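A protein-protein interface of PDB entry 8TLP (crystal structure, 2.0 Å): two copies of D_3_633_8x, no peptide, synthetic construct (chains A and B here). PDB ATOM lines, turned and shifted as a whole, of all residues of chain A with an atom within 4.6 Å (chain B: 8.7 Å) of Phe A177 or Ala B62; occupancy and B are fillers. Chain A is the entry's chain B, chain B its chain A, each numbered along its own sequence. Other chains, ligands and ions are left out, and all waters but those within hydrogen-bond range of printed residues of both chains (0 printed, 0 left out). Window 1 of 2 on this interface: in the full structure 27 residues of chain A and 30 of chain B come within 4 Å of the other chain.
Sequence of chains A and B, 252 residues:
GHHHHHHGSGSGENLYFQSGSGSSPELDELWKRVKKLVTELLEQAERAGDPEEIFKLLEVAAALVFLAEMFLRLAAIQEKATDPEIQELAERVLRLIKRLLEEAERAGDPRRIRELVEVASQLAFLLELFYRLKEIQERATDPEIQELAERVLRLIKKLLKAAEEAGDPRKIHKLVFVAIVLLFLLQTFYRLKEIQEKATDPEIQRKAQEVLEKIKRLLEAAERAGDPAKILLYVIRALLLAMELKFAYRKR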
ATOM      1  N   HIS A 173     -17.767 -15.992   2.277  1.00  0.00           N
ATOM      2  CA  HIS A 173     -17.276 -16.278   0.935  1.00  0.00           C
ATOM      3  C   HIS A 173     -15.964 -17.051   0.976  1.00  0.00           C
ATOM      4  O   HIS A 173     -15.730 -17.927   0.136  1.00  0.00           O
ATOM      5  CB  HIS A 173     -17.083 -14.980   0.152  1.00  0.00           C
ATOM      6  CG  HIS A 173     -16.023 -15.082  -0.896  1.00  0.00           C
ATOM      7  ND1 HIS A 173     -16.240 -15.695  -2.114  1.00  0.00           N
ATOM      8  CD2 HIS A 173     -14.724 -14.702  -0.890  1.00  0.00           C
ATOM      9  CE1 HIS A 173     -15.123 -15.666  -2.822  1.00  0.00           C
ATOM     10  NE2 HIS A 173     -14.188 -15.071  -2.101  1.00  0.00           N
ATOM     11  N   LYS A 174     -15.076 -16.715   1.920  1.00  0.00           N
ATOM     12  CA  LYS A 174     -13.793 -17.404   1.980  1.00  0.00           C
ATOM     13  C   LYS A 174     -13.975 -18.841   2.445  1.00  0.00           C
ATOM     14  O   LYS A 174     -13.470 -19.780   1.819  1.00  0.00           O
ATOM     15  CB  LYS A 174     -12.829 -16.654   2.897  1.00  0.00           C
ATOM     16  CG  LYS A 174     -12.218 -15.418   2.272  1.00  0.00           C
ATOM     17  CD  LYS A 174     -11.040 -14.892   3.103  1.00  0.00           C
ATOM     18  CE  LYS A 174     -11.406 -13.618   3.847  1.00  0.00           C
ATOM     19  NZ  LYS A 174     -11.728 -12.481   2.938  1.00  0.00           N
ATOM     20  N   LEU A 175     -14.721 -19.028   3.535  1.00  0.00           N
ATOM     21  CA  LEU A 175     -14.983 -20.365   4.048  1.00  0.00           C
ATOM     22  C   LEU A 175     -15.713 -21.212   3.017  1.00  0.00           C
ATOM     23  O   LEU A 175     -15.423 -22.407   2.864  1.00  0.00           O
ATOM     24  CB  LEU A 175     -15.796 -20.266   5.346  1.00  0.00           C
ATOM     25  CG  LEU A 175     -15.043 -19.539   6.469  1.00  0.00           C
ATOM     26  CD1 LEU A 175     -15.978 -18.955   7.553  1.00  0.00           C
ATOM     27  CD2 LEU A 175     -13.982 -20.454   7.082  1.00  0.00           C
ATOM     28  N   VAL A 176     -16.671 -20.614   2.306  1.00  0.00           N
ATOM     29  CA  VAL A 176     -17.413 -21.352   1.298  1.00  0.00           C
ATOM     30  C   VAL A 176     -16.505 -21.703   0.135  1.00  0.00           C
ATOM     31  O   VAL A 176     -16.619 -22.783  -0.455  1.00  0.00           O
ATOM     32  CB  VAL A 176     -18.646 -20.552   0.847  1.00  0.00           C
ATOM     33  CG1 VAL A 176     -19.170 -21.058  -0.510  1.00  0.00           C
ATOM     34  CG2 VAL A 176     -19.714 -20.650   1.911  1.00  0.00           C
ATOM     35  N   PHE A 177     -15.557 -20.826  -0.181  1.00  0.00           N
ATOM     36  CA  PHE A 177     -14.670 -21.099  -1.299  1.00  0.00           C
ATOM     37  C   PHE A 177     -13.782 -22.309  -1.027  1.00  0.00           C
ATOM     38  O   PHE A 177     -13.544 -23.139  -1.920  1.00  0.00           O
ATOM     39  CB  PHE A 177     -13.816 -19.882  -1.587  1.00  0.00           C
ATOM     40  CG  PHE A 177     -13.077 -19.990  -2.864  1.00  0.00           C
ATOM     41  CD1 PHE A 177     -13.689 -19.645  -4.056  1.00  0.00           C
ATOM     42  CD2 PHE A 177     -11.780 -20.480  -2.886  1.00  0.00           C
ATOM     43  CE1 PHE A 177     -12.991 -19.768  -5.262  1.00  0.00           C
ATOM     44  CE2 PHE A 177     -11.087 -20.606  -4.080  1.00  0.00           C
ATOM     45  CZ  PHE A 177     -11.689 -20.252  -5.263  1.00  0.00           C
ATOM     46  N   VAL A 178     -13.249 -22.405   0.189  1.00  0.00           N
ATOM     47  CA  VAL A 178     -12.450 -23.573   0.539  1.00  0.00           C
ATOM     48  C   VAL A 178     -13.310 -24.828   0.500  1.00  0.00           C
ATOM     49  O   VAL A 178     -12.895 -25.866  -0.032  1.00  0.00           O
ATOM     50  CB  VAL A 178     -11.791 -23.386   1.918  1.00  0.00           C
ATOM     51  CG1 VAL A 178     -11.018 -24.643   2.276  1.00  0.00           C
ATOM     52  CG2 VAL A 178     -10.883 -22.172   1.924  1.00  0.00           C
ATOM     53  N   ALA A 179     -14.534 -24.749   1.040  1.00  0.00           N
ATOM     54  CA  ALA A 179     -15.430 -25.902   1.001  1.00  0.00           C
ATOM     55  C   ALA A 179     -15.699 -26.354  -0.432  1.00  0.00           C
ATOM     56  O   ALA A 179     -15.715 -27.562  -0.719  1.00  0.00           O
ATOM     57  CB  ALA A 179     -16.744 -25.593   1.733  1.00  0.00           C
ATOM     58  N   ILE A 180     -15.915 -25.406  -1.346  1.00  0.00           N
ATOM     59  CA  ILE A 180     -16.133 -25.750  -2.759  1.00  0.00           C
ATOM     60  C   ILE A 180     -14.939 -26.511  -3.326  1.00  0.00           C
ATOM     61  O   ILE A 180     -15.098 -27.506  -4.044  1.00  0.00           O
ATOM     62  CB  ILE A 180     -16.387 -24.472  -3.583  1.00  0.00           C
ATOM     63  CG1 ILE A 180     -17.772 -23.880  -3.301  1.00  0.00           C
ATOM     64  CG2 ILE A 180     -16.204 -24.735  -5.085  1.00  0.00           C
ATOM     65  CD1 ILE A 180     -17.948 -22.453  -3.927  1.00  0.00           C
ATOM     66  N   VAL A 181     -13.730 -25.980  -3.112  1.00  0.00           N
ATOM     67  CA  VAL A 181     -12.538 -26.599  -3.690  1.00  0.00           C
ATOM     68  C   VAL A 181     -12.249 -27.932  -3.005  1.00  0.00           C
ATOM     69  O   VAL A 181     -11.766 -28.881  -3.639  1.00  0.00           O
ATOM     70  CB  VAL A 181     -11.343 -25.632  -3.586  1.00  0.00           C
ATOM     71  CG1 VAL A 181     -10.126 -26.255  -4.197  1.00  0.00           C
ATOM     72  CG2 VAL A 181     -11.655 -24.340  -4.321  1.00  0.00           C
ATOM     73  N   LEU A 232      -6.721 -24.232   2.096  1.00  0.00           N
ATOM     74  CA  LEU A 232      -6.835 -24.018   0.654  1.00  0.00           C
ATOM     75  C   LEU A 232      -5.541 -24.367  -0.074  1.00  0.00           C
ATOM     76  O   LEU A 232      -5.570 -24.994  -1.140  1.00  0.00           O
ATOM     77  CB  LEU A 232      -7.233 -22.570   0.371  1.00  0.00           C
ATOM     78  CG  LEU A 232      -7.668 -22.211  -1.053  1.00  0.00           C
ATOM     79  CD1 LEU A 232      -8.718 -23.209  -1.531  1.00  0.00           C
ATOM     80  CD2 LEU A 232      -8.225 -20.792  -1.090  1.00  0.00           C
ATOM     81  N   ILE A 236      -5.199 -27.072  -3.048  1.00  0.00           N
ATOM     82  CA  ILE A 236      -4.766 -26.735  -4.412  1.00  0.00           C
ATOM     83  C   ILE A 236      -3.552 -27.571  -4.821  1.00  0.00           C
ATOM     84  O   ILE A 236      -3.451 -28.030  -5.969  1.00  0.00           O
ATOM     85  CB  ILE A 236      -4.478 -25.231  -4.546  1.00  0.00           C
ATOM     86  CG1 ILE A 236      -5.735 -24.416  -4.243  1.00  0.00           C
ATOM     87  CG2 ILE A 236      -4.044 -24.916  -5.937  1.00  0.00           C
ATOM     88  CD1 ILE A 236      -5.474 -22.963  -4.168  1.00  0.00           C
ATOM     89  N   VAL B  34      -1.123 -23.322 -17.939  1.00  0.00           N
ATOM     90  CA  VAL B  34      -1.856 -23.284 -16.669  1.00  0.00           C
ATOM     91  C   VAL B  34      -0.973 -23.806 -15.547  1.00  0.00           C
ATOM     92  O   VAL B  34      -0.909 -23.217 -14.465  1.00  0.00           O
ATOM     93  CB  VAL B  34      -3.180 -24.075 -16.759  1.00  0.00           C
ATOM     94  CG1 VAL B  34      -3.745 -24.334 -15.356  1.00  0.00           C
ATOM     95  CG2 VAL B  34      -4.215 -23.325 -17.608  1.00  0.00           C
ATOM     96  N   LEU B  37       1.521 -21.001 -14.489  1.00  0.00           N
ATOM     97  CA  LEU B  37       0.921 -19.918 -13.720  1.00  0.00           C
ATOM     98  C   LEU B  37       0.479 -20.380 -12.334  1.00  0.00           C
ATOM     99  O   LEU B  37       0.590 -19.615 -11.367  1.00  0.00           O
ATOM    100  CB  LEU B  37      -0.256 -19.321 -14.490  1.00  0.00           C
ATOM    101  CG  LEU B  37      -0.056 -17.874 -14.943  1.00  0.00           C
ATOM    102  CD1 LEU B  37      -1.359 -17.311 -15.493  1.00  0.00           C
ATOM    103  CD2 LEU B  37       0.473 -17.004 -13.799  1.00  0.00           C
ATOM    104  N   VAL B  38      -0.027 -21.609 -12.209  1.00  0.00           N
ATOM    105  CA  VAL B  38      -0.465 -22.082 -10.900  1.00  0.00           C
ATOM    106  C   VAL B  38       0.717 -22.152  -9.940  1.00  0.00           C
ATOM    107  O   VAL B  38       0.650 -21.658  -8.807  1.00  0.00           O
ATOM    108  CB  VAL B  38      -1.163 -23.448 -11.011  1.00  0.00           C
ATOM    109  CG1 VAL B  38      -1.327 -24.050  -9.613  1.00  0.00           C
ATOM    110  CG2 VAL B  38      -2.513 -23.331 -11.708  1.00  0.00           C
ATOM    111  N   LEU B  41       1.790 -18.886  -8.657  1.00  0.00           N
ATOM    112  CA  LEU B  41       0.885 -18.358  -7.652  1.00  0.00           C
ATOM    113  C   LEU B  41       1.009 -19.129  -6.344  1.00  0.00           C
ATOM    114  O   LEU B  41       0.829 -18.554  -5.268  1.00  0.00           O
ATOM    115  CB  LEU B  41      -0.554 -18.397  -8.164  1.00  0.00           C
ATOM    116  CG  LEU B  41      -0.948 -17.378  -9.232  1.00  0.00           C
ATOM    117  CD1 LEU B  41      -2.109 -17.931  -9.989  1.00  0.00           C
ATOM    118  CD2 LEU B  41      -1.301 -16.018  -8.612  1.00  0.00           C
ATOM    119  N   LEU B  42       1.263 -20.443  -6.419  1.00  0.00           N
ATOM    120  CA  LEU B  42       1.470 -21.220  -5.197  1.00  0.00           C
ATOM    121  C   LEU B  42       2.735 -20.769  -4.479  1.00  0.00           C
ATOM    122  O   LEU B  42       2.739 -20.607  -3.251  1.00  0.00           O
ATOM    123  CB  LEU B  42       1.547 -22.714  -5.511  1.00  0.00           C
ATOM    124  CG  LEU B  42       0.241 -23.439  -5.818  1.00  0.00           C
ATOM    125  CD1 LEU B  42       0.491 -24.941  -5.977  1.00  0.00           C
ATOM    126  CD2 LEU B  42      -0.789 -23.146  -4.734  1.00  0.00           C
ATOM    127  N   PHE B  55      -4.970 -15.525   0.259  1.00  0.00           N
ATOM    128  CA  PHE B  55      -6.219 -16.144  -0.159  1.00  0.00           C
ATOM    129  C   PHE B  55      -6.618 -15.687  -1.553  1.00  0.00           C
ATOM    130  O   PHE B  55      -7.160 -16.475  -2.333  1.00  0.00           O
ATOM    131  CB  PHE B  55      -7.326 -15.830   0.839  1.00  0.00           C
ATOM    132  CG  PHE B  55      -8.470 -16.815   0.808  1.00  0.00           C
ATOM    133  CD1 PHE B  55      -8.566 -17.822   1.762  1.00  0.00           C
ATOM    134  CD2 PHE B  55      -9.444 -16.738  -0.173  1.00  0.00           C
ATOM    135  CE1 PHE B  55      -9.620 -18.722   1.739  1.00  0.00           C
ATOM    136  CE2 PHE B  55     -10.492 -17.638  -0.204  1.00  0.00           C
ATOM    137  CZ  PHE B  55     -10.581 -18.629   0.749  1.00  0.00           C
ATOM    138  N   LYS B  56      -6.345 -14.425  -1.894  1.00  0.00           N
ATOM    139  CA  LYS B  56      -6.694 -13.955  -3.227  1.00  0.00           C
ATOM    140  C   LYS B  56      -5.791 -14.577  -4.276  1.00  0.00           C
ATOM    141  O   LYS B  56      -6.260 -14.949  -5.358  1.00  0.00           O
ATOM    142  CB  LYS B  56      -6.670 -12.426  -3.277  1.00  0.00           C
ATOM    143  CG  LYS B  56      -7.940 -11.841  -2.660  1.00  0.00           C
ATOM    144  CD  LYS B  56      -8.031 -10.321  -2.776  1.00  0.00           C
ATOM    145  N   LEU B  57      -4.510 -14.755  -3.965  1.00  0.00           N
ATOM    146  CA  LEU B  57      -3.646 -15.506  -4.866  1.00  0.00           C
ATOM    147  C   LEU B  57      -4.155 -16.930  -5.048  1.00  0.00           C
ATOM    148  O   LEU B  57      -4.154 -17.463  -6.166  1.00  0.00           O
ATOM    149  CB  LEU B  57      -2.216 -15.542  -4.328  1.00  0.00           C
ATOM    150  CG  LEU B  57      -1.494 -14.198  -4.250  1.00  0.00           C
ATOM    151  CD1 LEU B  57      -0.372 -14.242  -3.231  1.00  0.00           C
ATOM    152  CD2 LEU B  57      -0.962 -13.844  -5.617  1.00  0.00           C
ATOM    153  N   LEU B  58      -4.585 -17.562  -3.953  1.00  0.00           N
ATOM    154  CA  LEU B  58      -5.031 -18.950  -4.015  1.00  0.00           C
ATOM    155  C   LEU B  58      -6.371 -19.086  -4.737  1.00  0.00           C
ATOM    156  O   LEU B  58      -6.628 -20.121  -5.363  1.00  0.00           O
ATOM    157  CB  LEU B  58      -5.113 -19.522  -2.600  1.00  0.00           C
ATOM    158  CG  LEU B  58      -3.768 -19.708  -1.886  1.00  0.00           C
ATOM    159  CD1 LEU B  58      -3.967 -20.305  -0.505  1.00  0.00           C
ATOM    160  CD2 LEU B  58      -2.889 -20.579  -2.717  1.00  0.00           C
ATOM    161  N   GLU B  59      -7.238 -18.072  -4.645  1.00  0.00           N
ATOM    162  CA  GLU B  59      -8.453 -18.052  -5.452  1.00  0.00           C
ATOM    163  C   GLU B  59      -8.130 -18.032  -6.936  1.00  0.00           C
ATOM    164  O   GLU B  59      -8.872 -18.609  -7.737  1.00  0.00           O
ATOM    165  CB  GLU B  59      -9.316 -16.837  -5.095  1.00  0.00           C
ATOM    166  CG  GLU B  59     -10.253 -17.050  -3.919  1.00  0.00           C
ATOM    167  CD  GLU B  59     -10.916 -15.754  -3.476  1.00  0.00           C
ATOM    168  OE1 GLU B  59     -10.225 -14.712  -3.428  1.00  0.00           O
ATOM    169  OE2 GLU B  59     -12.126 -15.764  -3.189  1.00  0.00           O
ATOM    170  N   VAL B  60      -7.032 -17.368  -7.326  1.00  0.00           N
ATOM    171  CA  VAL B  60      -6.611 -17.371  -8.725  1.00  0.00           C
ATOM    172  C   VAL B  60      -6.067 -18.742  -9.119  1.00  0.00           C
ATOM    173  O   VAL B  60      -6.439 -19.289 -10.163  1.00  0.00           O
ATOM    174  CB  VAL B  60      -5.586 -16.243  -8.981  1.00  0.00           C
ATOM    175  CG1 VAL B  60      -5.138 -16.227 -10.427  1.00  0.00           C
ATOM    176  CG2 VAL B  60      -6.181 -14.893  -8.625  1.00  0.00           C
ATOM    177  N   ALA B  61      -5.198 -19.335  -8.294  1.00  0.00           N
ATOM    178  CA  ALA B  61      -4.692 -20.666  -8.628  1.00  0.00           C
ATOM    179  C   ALA B  61      -5.824 -21.685  -8.723  1.00  0.00           C
ATOM    180  O   ALA B  61      -5.798 -22.567  -9.590  1.00  0.00           O
ATOM    181  CB  ALA B  61      -3.652 -21.124  -7.603  1.00  0.00           C
ATOM    182  N   ALA B  62      -6.813 -21.591  -7.826  1.00  0.00           N
ATOM    183  CA  ALA B  62      -7.954 -22.502  -7.846  1.00  0.00           C
ATOM    184  C   ALA B  62      -8.748 -22.361  -9.137  1.00  0.00           C
ATOM    185  O   ALA B  62      -9.114 -23.361  -9.768  1.00  0.00           O
ATOM    186  CB  ALA B  62      -8.869 -22.238  -6.636  1.00  0.00           C
ATOM    187  N   ALA B  63      -9.074 -21.122  -9.514  1.00  0.00           N
ATOM    188  CA  ALA B  63      -9.750 -20.877 -10.780  1.00  0.00           C
ATOM    189  C   ALA B  63      -8.944 -21.419 -11.953  1.00  0.00           C
ATOM    190  O   ALA B  63      -9.526 -21.888 -12.936  1.00  0.00           O
ATOM    191  CB  ALA B  63     -10.023 -19.369 -10.957  1.00  0.00           C
ATOM    192  N   LEU B  64      -7.609 -21.364 -11.876  1.00  0.00           N
ATOM    193  CA  LEU B  64      -6.790 -21.928 -12.943  1.00  0.00           C
ATOM    194  C   LEU B  64      -6.931 -23.448 -13.015  1.00  0.00           C
ATOM    195  O   LEU B  64      -6.971 -24.027 -14.106  1.00  0.00           O
ATOM    196  CB  LEU B  64      -5.337 -21.532 -12.725  1.00  0.00           C
ATOM    197  CG  LEU B  64      -4.939 -20.144 -13.216  1.00  0.00           C
ATOM    198  CD1 LEU B  64      -3.590 -19.777 -12.677  1.00  0.00           C
ATOM    199  CD2 LEU B  64      -4.933 -20.123 -14.735  1.00  0.00           C
ATOM    200  N   VAL B  65      -7.024 -24.113 -11.861  1.00  0.00           N
ATOM    201  CA  VAL B  65      -7.220 -25.560 -11.847  1.00  0.00           C
ATOM    202  C   VAL B  65      -8.611 -25.928 -12.369  1.00  0.00           C
ATOM    203  O   VAL B  65      -8.784 -26.954 -13.039  1.00  0.00           O
ATOM    204  CB  VAL B  65      -6.978 -26.104 -10.426  1.00  0.00           C
ATOM    205  CG1 VAL B  65      -7.226 -27.593 -10.383  1.00  0.00           C
ATOM    206  CG2 VAL B  65      -5.550 -25.788  -9.970  1.00  0.00           C
ATOM    207  N   PHE B  66      -9.628 -25.132 -12.032  1.00  0.00           N
ATOM    208  CA  PHE B  66     -10.947 -25.323 -12.615  1.00  0.00           C
ATOM    209  C   PHE B  66     -10.885 -25.216 -14.130  1.00  0.00           C
ATOM    210  O   PHE B  66     -11.540 -25.982 -14.839  1.00  0.00           O
ATOM    211  CB  PHE B  66     -11.931 -24.297 -12.057  1.00  0.00           C
ATOM    212  CG  PHE B  66     -13.180 -24.130 -12.895  1.00  0.00           C
ATOM    213  CD2 PHE B  66     -13.303 -23.069 -13.798  1.00  0.00           C
ATOM    214  CE2 PHE B  66     -14.450 -22.896 -14.587  1.00  0.00           C
ATOM    215  CZ  PHE B  66     -15.525 -23.773 -14.490  1.00  0.00           C
ATOM    216  N   LEU B  67     -10.111 -24.249 -14.634  1.00  0.00           N
ATOM    217  CA  LEU B  67      -9.882 -24.104 -16.066  1.00  0.00           C
ATOM    218  C   LEU B  67      -9.393 -25.404 -16.679  1.00  0.00           C
ATOM    219  O   LEU B  67      -9.947 -25.885 -17.677  1.00  0.00           O
ATOM    220  CB  LEU B  67      -8.859 -22.994 -16.303  1.00  0.00           C
ATOM    221  CG  LEU B  67      -9.374 -21.661 -16.819  1.00  0.00           C
ATOM    222  CD1 LEU B  67      -8.242 -20.653 -16.970  1.00  0.00           C
ATOM    223  CD2 LEU B  67      -9.982 -21.953 -18.148  1.00  0.00           C
ATOM    224  N   ALA B  68      -8.325 -25.970 -16.110  1.00  0.00           N
ATOM    225  CA  ALA B  68      -7.816 -27.242 -16.589  1.00  0.00           C
ATOM    226  C   ALA B  68      -8.873 -28.342 -16.536  1.00  0.00           C
ATOM    227  O   ALA B  68      -8.898 -29.214 -17.411  1.00  0.00           O
ATOM    228  CB  ALA B  68      -6.586 -27.638 -15.780  1.00  0.00           C
ATOM    229  N   GLU B  69      -9.738 -28.334 -15.519  1.00  0.00           N
ATOM    230  CA  GLU B  69     -10.816 -29.319 -15.467  1.00  0.00           C
ATOM    231  C   GLU B  69     -11.780 -29.125 -16.626  1.00  0.00           C
ATOM    232  O   GLU B  69     -12.283 -30.099 -17.203  1.00  0.00           O
ATOM    233  CB  GLU B  69     -11.555 -29.228 -14.133  1.00  0.00           C
ATOM    234  CG  GLU B  69     -12.806 -30.103 -14.041  1.00  0.00           C
ATOM    235  CD  GLU B  69     -12.498 -31.596 -13.860  1.00  0.00           C
ATOM    236  OE1 GLU B  69     -11.310 -31.983 -13.847  1.00  0.00           O
ATOM    237  OE2 GLU B  69     -13.450 -32.388 -13.715  1.00  0.00           O
ATOM    238  N   VAL B 117      -7.812 -14.011 -15.127  1.00  0.00           N
ATOM    239  CA  VAL B 117      -8.107 -15.410 -14.846  1.00  0.00           C
ATOM    240  C   VAL B 117      -9.601 -15.605 -14.611  1.00  0.00           C
ATOM    241  O   VAL B 117     -10.182 -16.604 -15.048  1.00  0.00           O
ATOM    242  CB  VAL B 117      -7.273 -15.887 -13.643  1.00  0.00           C
ATOM    243  CG1 VAL B 117      -7.886 -17.145 -13.008  1.00  0.00           C
ATOM    244  CG2 VAL B 117      -5.837 -16.128 -14.053  1.00  0.00           C
ATOM    245  N   GLU B 118     -10.247 -14.651 -13.938  1.00  0.00           N
ATOM    246  CA  GLU B 118     -11.674 -14.765 -13.676  1.00  0.00           C
ATOM    247  C   GLU B 118     -12.460 -14.854 -14.974  1.00  0.00           C
ATOM    248  O   GLU B 118     -13.372 -15.679 -15.101  1.00  0.00           O
ATOM    249  CB  GLU B 118     -12.166 -13.576 -12.848  1.00  0.00           C
ATOM    250  CG  GLU B 118     -11.904 -13.709 -11.366  1.00  0.00           C
ATOM    251  CD  GLU B 118     -12.037 -12.385 -10.622  1.00  0.00           C
ATOM    252  OE2 GLU B 118     -13.189 -11.933 -10.427  1.00  0.00           O
ATOM    253  N   SER B 121     -11.953 -18.137 -16.665  1.00  0.00           N
ATOM    254  CA  SER B 121     -12.679 -19.257 -16.077  1.00  0.00           C
ATOM    255  C   SER B 121     -14.178 -19.192 -16.386  1.00  0.00           C
ATOM    256  O   SER B 121     -14.829 -20.236 -16.450  1.00  0.00           O
ATOM    257  CB  SER B 121     -12.426 -19.305 -14.571  1.00  0.00           C
ATOM    258  OG  SER B 121     -13.269 -18.406 -13.893  1.00  0.00           O
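OE2 of Glu B59 is in hydrogen-bond range of NE2 of His A173.
O of Lys A174 touches CZ of Phe B55, 3.3 Å away.
Phe A177 touches Glu B59.
Phe A177 touches Ala B62 (CZ to CB, 3.7 Å).
CE1 of Phe B55 touches CG2 of Val A178 (3.7 Å).
CD2 of Leu A232 touches CZ of Phe B55, 3.7 Å away.
CD2 of Leu A232 touches CB of Leu B58, at 3.7 Å.
Ile A236 touches Leu B42.
CD1 of Ile A236 touches O of Leu B58, at 3.3 Å.
Of chain B, only Glu B59 and Ala B62 come within 4 Å of Phe A177.
Printed residues of chain A within 4 Å of Ala B62: Phe A177 (3.7 Å).
Of the printed residues of chain B, Leu A232 touches Phe B55 and Leu B58.
Printed residues of chain A within 4 Å of Glu B59: His A173 and Phe A177.
Of the printed residues of chain B, Val A178 touches Phe B55 (3.7 Å).
Glu B118 touches none of the printed residues of chain A.
Leu B41 touches none of the printed residues of chain A.
The nearest residue of chain A that does not touch Ala B62 is Ile A236 (4.1 Å).
Hydrophobic or aromatic side chains of chain A within 4 Å of the printed part of chain B: His A173, Phe A177, Val A178, Leu A232 and Ile A236.
Of the 23 printed residues of chain B, 5 touch a printed residue of chain A.
Printed residues of chain B that touch a printed residue of chain A: Leu B42, Phe B55, Leu B58, Glu B59 and Ala B62.
Hydrophobic or aromatic side chains of chain B within 4 Å of the printed part of chain A: Leu B42, Phe B55, Leu B58 and Ala B62.
Along chain B the printed residues that touch a printed residue of chain A span positions 42 to 62.
Among the printed residues, 9 pairs touch across the chains.
No position is printed for both chains.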
